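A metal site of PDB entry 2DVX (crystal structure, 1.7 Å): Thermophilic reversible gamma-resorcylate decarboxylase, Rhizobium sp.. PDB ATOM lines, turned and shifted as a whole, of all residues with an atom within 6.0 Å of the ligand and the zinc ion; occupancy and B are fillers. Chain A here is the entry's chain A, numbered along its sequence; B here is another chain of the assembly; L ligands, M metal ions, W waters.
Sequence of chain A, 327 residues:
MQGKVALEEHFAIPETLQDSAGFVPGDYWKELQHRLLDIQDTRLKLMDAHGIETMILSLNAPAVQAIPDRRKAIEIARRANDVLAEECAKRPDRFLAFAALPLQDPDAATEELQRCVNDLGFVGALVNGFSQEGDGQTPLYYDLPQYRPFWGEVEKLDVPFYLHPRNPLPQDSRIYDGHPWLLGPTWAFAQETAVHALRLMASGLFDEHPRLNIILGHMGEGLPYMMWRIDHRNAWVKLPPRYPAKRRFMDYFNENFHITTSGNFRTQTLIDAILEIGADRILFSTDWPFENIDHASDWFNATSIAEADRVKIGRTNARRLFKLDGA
The side-chain carboxylate (OE2) of Glu 291 lies within hydrogen-bond range of the backbone NH (N) of Asn 234 of chain B (2.7 Å).
The side-chain hydroxyl (OG) of Ser 262 lies within hydrogen-bond range of the side-chain carboxylate (OE2) of Glu 8, 2.6 Å away.
O of Phe 290 sits close to OD1 of Asn 234 of chain B, 2.9 Å away.
OE1 of Glu 8 lies close to NE2 of His 218 (3.2 Å).
A ring nitrogen (NE2) of His 218 is in hydrogen-bond range of the side-chain carboxylate (OD2) of Asp 287.
The backbone carbonyl oxygen (O) of Gly 184 is in hydrogen-bond range of the backbone NH (N) of Phe 189 (2.9 Å).
Phe 23 touches the ligand (CG to C7, 3.3 Å).
CD of Pro 185 touches O3 of the ligand, 3.5 Å away.
Phe 189 touches the ligand (CE1 to C5, 3.9 Å).
Phe 290 touches the ligand.
OD1 of Asn 234 of chain B touches O2 of the ligand, 3.6 Å away.
Hydrophobic or aromatic side chains within 4 Å of the ligand: His 10, Phe 23, His 164, Pro 185, Phe 189 and Phe 290.
The nearest printed residue that does not touch the ligand is Ala 61 (4.5 Å).
An oxygen (O1) of the ligand binds the zinc ion (1.9 Å).
The side-chain carboxylate (OE1) of Glu 8 is bound to the zinc ion.
The zinc ion is bound by NE2 of His 164 (2.1 Å).
A ring nitrogen (NE2) of His 10 is bound to the zinc ion (2.2 Å).
The side-chain carboxylate (OD1) of Asp 287 is bound to the zinc ion (2.3 Å).
Water W2 lies within hydrogen-bond range of the guanidinium group of Arg 229 of chain B, an oxygen (O2) of the ligand, the side-chain carboxylate of Asp 287 and a ring nitrogen (NE2) of His 218.
Water W1 lies within hydrogen-bond range of OG of Ser 20 (2.5 Å) and O of Ala 61 (2.7 Å).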
ATOM      1  N   GLU A   8     -11.053  19.820  20.750  1.00  0.00           N
ATOM      2  CA  GLU A   8     -11.382  21.238  20.784  1.00  0.00           C
ATOM      3  C   GLU A   8     -12.876  21.190  20.481  1.00  0.00           C
ATOM      4  O   GLU A   8     -13.332  21.545  19.405  1.00  0.00           O
ATOM      5  CB  GLU A   8     -10.653  22.095  19.747  1.00  0.00           C
ATOM      6  CG  GLU A   8     -10.940  23.589  20.042  1.00  0.00           C
ATOM      7  CD  GLU A   8     -10.240  24.588  19.140  1.00  0.00           C
ATOM      8  OE1 GLU A   8     -10.834  25.661  18.908  1.00  0.00           O
ATOM      9  OE2 GLU A   8      -9.113  24.337  18.671  1.00  0.00           O
ATOM     10  N   HIS A  10     -16.404  22.271  22.245  1.00  0.00           N
ATOM     11  CA  HIS A  10     -16.959  23.164  23.252  1.00  0.00           C
ATOM     12  C   HIS A  10     -18.402  22.970  23.684  1.00  0.00           C
ATOM     13  O   HIS A  10     -19.208  22.332  23.009  1.00  0.00           O
ATOM     14  CB  HIS A  10     -16.793  24.599  22.771  1.00  0.00           C
ATOM     15  CG  HIS A  10     -15.408  24.919  22.286  1.00  0.00           C
ATOM     16  ND1 HIS A  10     -14.327  25.003  23.128  1.00  0.00           N
ATOM     17  CD2 HIS A  10     -14.942  25.166  21.036  1.00  0.00           C
ATOM     18  CE1 HIS A  10     -13.244  25.297  22.428  1.00  0.00           C
ATOM     19  NE2 HIS A  10     -13.587  25.402  21.152  1.00  0.00           N
ATOM     20  N   ASP A  19     -21.634  34.746  25.331  1.00  0.00           N
ATOM     21  CA  ASP A  19     -20.314  35.008  24.791  1.00  0.00           C
ATOM     22  C   ASP A  19     -20.203  34.523  23.342  1.00  0.00           C
ATOM     23  O   ASP A  19     -19.398  35.051  22.564  1.00  0.00           O
ATOM     24  CB  ASP A  19     -19.244  34.294  25.629  1.00  0.00           C
ATOM     25  CG  ASP A  19     -18.802  35.115  26.822  1.00  0.00           C
ATOM     26  OD1 ASP A  19     -19.588  35.959  27.310  1.00  0.00           O
ATOM     27  OD2 ASP A  19     -17.661  34.912  27.282  1.00  0.00           O
ATOM     28  N   SER A  20     -21.009  33.527  22.981  1.00  0.00           N
ATOM     29  CA  SER A  20     -20.992  32.966  21.634  1.00  0.00           C
ATOM     30  C   SER A  20     -22.024  33.552  20.679  1.00  0.00           C
ATOM     31  O   SER A  20     -22.017  33.237  19.486  1.00  0.00           O
ATOM     32  CB  SER A  20     -21.190  31.443  21.711  1.00  0.00           C
ATOM     33  OG  SER A  20     -20.181  30.833  22.489  1.00  0.00           O
ATOM     34  N   PHE A  23     -21.017  35.401  17.160  1.00  0.00           N
ATOM     35  CA  PHE A  23     -20.198  34.728  16.156  1.00  0.00           C
ATOM     36  C   PHE A  23     -20.982  33.898  15.148  1.00  0.00           C
ATOM     37  O   PHE A  23     -20.409  33.072  14.428  1.00  0.00           O
ATOM     38  CB  PHE A  23     -19.135  33.868  16.835  1.00  0.00           C
ATOM     39  CG  PHE A  23     -18.158  34.673  17.662  1.00  0.00           C
ATOM     40  CD1 PHE A  23     -18.465  35.036  18.969  1.00  0.00           C
ATOM     41  CD2 PHE A  23     -16.937  35.057  17.127  1.00  0.00           C
ATOM     42  CE1 PHE A  23     -17.572  35.774  19.734  1.00  0.00           C
ATOM     43  CE2 PHE A  23     -16.022  35.793  17.889  1.00  0.00           C
ATOM     44  CZ  PHE A  23     -16.339  36.152  19.197  1.00  0.00           C
ATOM     45  N   VAL A  24     -22.292  34.119  15.099  1.00  0.00           N
ATOM     46  CA  VAL A  24     -23.174  33.435  14.155  1.00  0.00           C
ATOM     47  C   VAL A  24     -24.367  34.351  13.887  1.00  0.00           C
ATOM     48  O   VAL A  24     -24.834  35.050  14.794  1.00  0.00           O
ATOM     49  CB  VAL A  24     -23.709  32.094  14.715  1.00  0.00           C
ATOM     50  CG1 VAL A  24     -22.553  31.107  14.873  1.00  0.00           C
ATOM     51  CG2 VAL A  24     -24.415  32.314  16.045  1.00  0.00           C
ATOM     52  N   ALA A  61     -15.706  30.380  24.526  1.00  0.00           N
ATOM     53  CA  ALA A  61     -14.846  31.551  24.661  1.00  0.00           C
ATOM     54  C   ALA A  61     -15.543  32.896  24.433  1.00  0.00           C
ATOM     55  O   ALA A  61     -16.543  32.975  23.718  1.00  0.00           O
ATOM     56  CB  ALA A  61     -13.675  31.423  23.688  1.00  0.00           C
ATOM     57  N   HIS A 164      -6.213  28.490  23.552  1.00  0.00           N
ATOM     58  CA  HIS A 164      -7.302  28.744  22.603  1.00  0.00           C
ATOM     59  C   HIS A 164      -7.422  30.234  22.273  1.00  0.00           C
ATOM     60  O   HIS A 164      -6.964  31.082  23.025  1.00  0.00           O
ATOM     61  CB  HIS A 164      -8.608  28.200  23.225  1.00  0.00           C
ATOM     62  CG  HIS A 164      -9.789  28.194  22.302  1.00  0.00           C
ATOM     63  ND1 HIS A 164     -10.583  29.298  22.109  1.00  0.00           N
ATOM     64  CD2 HIS A 164     -10.304  27.204  21.530  1.00  0.00           C
ATOM     65  CE1 HIS A 164     -11.540  28.994  21.247  1.00  0.00           C
ATOM     66  NE2 HIS A 164     -11.398  27.732  20.883  1.00  0.00           N
ATOM     67  N   PRO A 165      -8.036  30.569  21.122  1.00  0.00           N
ATOM     68  CA  PRO A 165      -8.189  31.981  20.743  1.00  0.00           C
ATOM     69  C   PRO A 165      -9.230  32.798  21.496  1.00  0.00           C
ATOM     70  O   PRO A 165     -10.079  32.273  22.219  1.00  0.00           O
ATOM     71  CB  PRO A 165      -8.567  31.907  19.264  1.00  0.00           C
ATOM     72  CG  PRO A 165      -8.046  30.575  18.808  1.00  0.00           C
ATOM     73  CD  PRO A 165      -8.348  29.692  19.984  1.00  0.00           C
ATOM     74  N   GLY A 184     -12.445  37.395  15.009  1.00  0.00           N
ATOM     75  CA  GLY A 184     -12.876  36.010  15.161  1.00  0.00           C
ATOM     76  C   GLY A 184     -12.071  34.994  14.370  1.00  0.00           C
ATOM     77  O   GLY A 184     -10.900  35.213  14.049  1.00  0.00           O
ATOM     78  N   PRO A 185     -12.692  33.856  14.013  1.00  0.00           N
ATOM     79  CA  PRO A 185     -12.040  32.781  13.271  1.00  0.00           C
ATOM     80  C   PRO A 185     -11.514  33.112  11.872  1.00  0.00           C
ATOM     81  O   PRO A 185     -10.668  32.375  11.346  1.00  0.00           O
ATOM     82  CB  PRO A 185     -13.113  31.680  13.244  1.00  0.00           C
ATOM     83  CG  PRO A 185     -14.374  32.468  13.221  1.00  0.00           C
ATOM     84  CD  PRO A 185     -14.122  33.534  14.250  1.00  0.00           C
ATOM     85  N   PHE A 189      -8.440  35.748  15.512  1.00  0.00           N
ATOM     86  CA  PHE A 189      -8.196  34.653  16.449  1.00  0.00           C
ATOM     87  C   PHE A 189      -6.787  34.067  16.281  1.00  0.00           C
ATOM     88  O   PHE A 189      -6.086  33.825  17.269  1.00  0.00           O
ATOM     89  CB  PHE A 189      -9.193  33.512  16.222  1.00  0.00           C
ATOM     90  CG  PHE A 189     -10.486  33.652  16.978  1.00  0.00           C
ATOM     91  CD1 PHE A 189     -11.433  32.631  16.916  1.00  0.00           C
ATOM     92  CD2 PHE A 189     -10.760  34.776  17.749  1.00  0.00           C
ATOM     93  CE1 PHE A 189     -12.642  32.728  17.622  1.00  0.00           C
ATOM     94  CE2 PHE A 189     -11.960  34.877  18.454  1.00  0.00           C
ATOM     95  CZ  PHE A 189     -12.907  33.855  18.391  1.00  0.00           C
ATOM     96  N   HIS A 218      -6.568  25.000  15.146  1.00  0.00           N
ATOM     97  CA  HIS A 218      -6.544  25.632  13.831  1.00  0.00           C
ATOM     98  C   HIS A 218      -5.212  25.496  13.119  1.00  0.00           C
ATOM     99  O   HIS A 218      -4.733  26.427  12.469  1.00  0.00           O
ATOM    100  CB  HIS A 218      -6.948  27.088  14.005  1.00  0.00           C
ATOM    101  CG  HIS A 218      -8.040  27.259  15.023  1.00  0.00           C
ATOM    102  ND1 HIS A 218      -7.797  27.705  16.308  1.00  0.00           N
ATOM    103  CD2 HIS A 218      -9.347  26.882  14.992  1.00  0.00           C
ATOM    104  CE1 HIS A 218      -8.903  27.595  17.027  1.00  0.00           C
ATOM    105  NE2 HIS A 218      -9.855  27.091  16.251  1.00  0.00           N
ATOM    106  N   SER A 262      -8.598  21.504  14.290  1.00  0.00           N
ATOM    107  CA  SER A 262      -9.834  22.233  14.512  1.00  0.00           C
ATOM    108  C   SER A 262     -10.061  23.376  13.538  1.00  0.00           C
ATOM    109  O   SER A 262      -9.182  24.203  13.302  1.00  0.00           O
ATOM    110  CB  SER A 262      -9.882  22.774  15.946  1.00  0.00           C
ATOM    111  OG  SER A 262      -8.876  23.747  16.166  1.00  0.00           O
ATOM    112  N   ASP A 287     -13.772  21.532  16.550  1.00  0.00           N
ATOM    113  CA  ASP A 287     -14.199  22.879  16.960  1.00  0.00           C
ATOM    114  C   ASP A 287     -15.725  22.912  17.000  1.00  0.00           C
ATOM    115  O   ASP A 287     -16.353  23.963  16.837  1.00  0.00           O
ATOM    116  CB  ASP A 287     -13.673  23.971  16.016  1.00  0.00           C
ATOM    117  CG  ASP A 287     -13.303  25.246  16.766  1.00  0.00           C
ATOM    118  OD1 ASP A 287     -13.663  25.350  17.960  1.00  0.00           O
ATOM    119  OD2 ASP A 287     -12.648  26.139  16.163  1.00  0.00           O
ATOM    120  N   PHE A 290     -19.030  25.036  16.623  1.00  0.00           N
ATOM    121  CA  PHE A 290     -18.783  26.117  15.672  1.00  0.00           C
ATOM    122  C   PHE A 290     -18.484  25.566  14.281  1.00  0.00           C
ATOM    123  O   PHE A 290     -18.594  26.272  13.274  1.00  0.00           O
ATOM    124  CB  PHE A 290     -17.639  26.989  16.194  1.00  0.00           C
ATOM    125  CG  PHE A 290     -17.921  27.567  17.550  1.00  0.00           C
ATOM    126  CD1 PHE A 290     -18.807  28.622  17.700  1.00  0.00           C
ATOM    127  CD2 PHE A 290     -17.335  27.016  18.693  1.00  0.00           C
ATOM    128  CE1 PHE A 290     -19.114  29.134  18.964  1.00  0.00           C
ATOM    129  CE2 PHE A 290     -17.639  27.519  19.957  1.00  0.00           C
ATOM    130  CZ  PHE A 290     -18.526  28.574  20.097  1.00  0.00           C
ATOM    131  N   GLU A 291     -18.105  24.296  14.237  1.00  0.00           N
ATOM    132  CA  GLU A 291     -17.845  23.574  12.988  1.00  0.00           C
ATOM    133  C   GLU A 291     -18.651  22.289  13.088  1.00  0.00           C
ATOM    134  O   GLU A 291     -18.817  21.747  14.174  1.00  0.00           O
ATOM    135  CB  GLU A 291     -16.363  23.189  12.862  1.00  0.00           C
ATOM    136  CG  GLU A 291     -15.398  24.353  12.788  1.00  0.00           C
ATOM    137  CD  GLU A 291     -15.561  25.193  11.535  1.00  0.00           C
ATOM    138  OE1 GLU A 291     -16.240  24.768  10.579  1.00  0.00           O
ATOM    139  OE2 GLU A 291     -14.978  26.297  11.505  1.00  0.00           O
ATOM    140  N   ARG B 229      -9.222  28.478   5.702  1.00  0.00           N
ATOM    141  CA  ARG B 229      -9.923  28.858   6.915  1.00  0.00           C
ATOM    142  C   ARG B 229     -10.528  30.263   6.841  1.00  0.00           C
ATOM    143  O   ARG B 229     -11.626  30.484   7.347  1.00  0.00           O
ATOM    144  CB  ARG B 229      -8.973  28.750   8.118  1.00  0.00           C
ATOM    145  CG  ARG B 229      -9.618  29.079   9.469  1.00  0.00           C
ATOM    146  CD  ARG B 229      -8.744  28.609  10.632  1.00  0.00           C
ATOM    147  NE  ARG B 229      -9.089  29.245  11.892  1.00  0.00           N
ATOM    148  CZ  ARG B 229     -10.186  28.999  12.610  1.00  0.00           C
ATOM    149  NH1 ARG B 229     -11.076  28.110  12.192  1.00  0.00           N
ATOM    150  NH2 ARG B 229     -10.391  29.634  13.746  1.00  0.00           N
ATOM    151  N   ASN B 234     -16.495  27.938  10.049  1.00  0.00           N
ATOM    152  CA  ASN B 234     -17.935  27.861  10.329  1.00  0.00           C
ATOM    153  C   ASN B 234     -18.740  27.637   9.050  1.00  0.00           C
ATOM    154  O   ASN B 234     -19.758  28.290   8.828  1.00  0.00           O
ATOM    155  CB  ASN B 234     -18.426  29.156  10.987  1.00  0.00           C
ATOM    156  CG  ASN B 234     -17.545  29.599  12.133  1.00  0.00           C
ATOM    157  OD1 ASN B 234     -17.192  28.812  12.997  1.00  0.00           O
ATOM    158  ND2 ASN B 234     -17.210  30.886  12.136  1.00  0.00           N
HETATM  159  C1  LIG L   1     -14.060  28.421  18.272  1.00  0.00           C
HETATM  160  O1  LIG L   1     -13.664  28.011  19.383  1.00  0.00           O
HETATM  161  C2  LIG L   1     -14.888  29.569  18.223  1.00  0.00           C
HETATM  162  C3  LIG L   1     -15.223  30.199  19.461  1.00  0.00           C
HETATM  163  C4  LIG L   1     -16.061  31.356  19.494  1.00  0.00           C
HETATM  164  C5  LIG L   1     -15.388  30.087  17.008  1.00  0.00           C
HETATM  165  O2  LIG L   1     -15.106  29.545  15.782  1.00  0.00           O
HETATM  166  C6  LIG L   1     -16.229  31.253  17.041  1.00  0.00           C
HETATM  167  C7  LIG L   1     -16.546  31.857  18.268  1.00  0.00           C
HETATM  168  O3  LIG L   1     -16.712  31.769  15.915  1.00  0.00           O
HETATM  169 ZN    ZN M   1     -12.564  26.490  19.604  1.00  0.00          ZN
HETATM  170  O   HOH W   1     -17.742  31.272  22.076  1.00  0.00           O
HETATM  171  O   HOH W   2     -12.259  29.251  15.823  1.00  0.00           O
HETATM  172  O   HOH W   3     -15.018  28.412  22.147  1.00  0.00           O
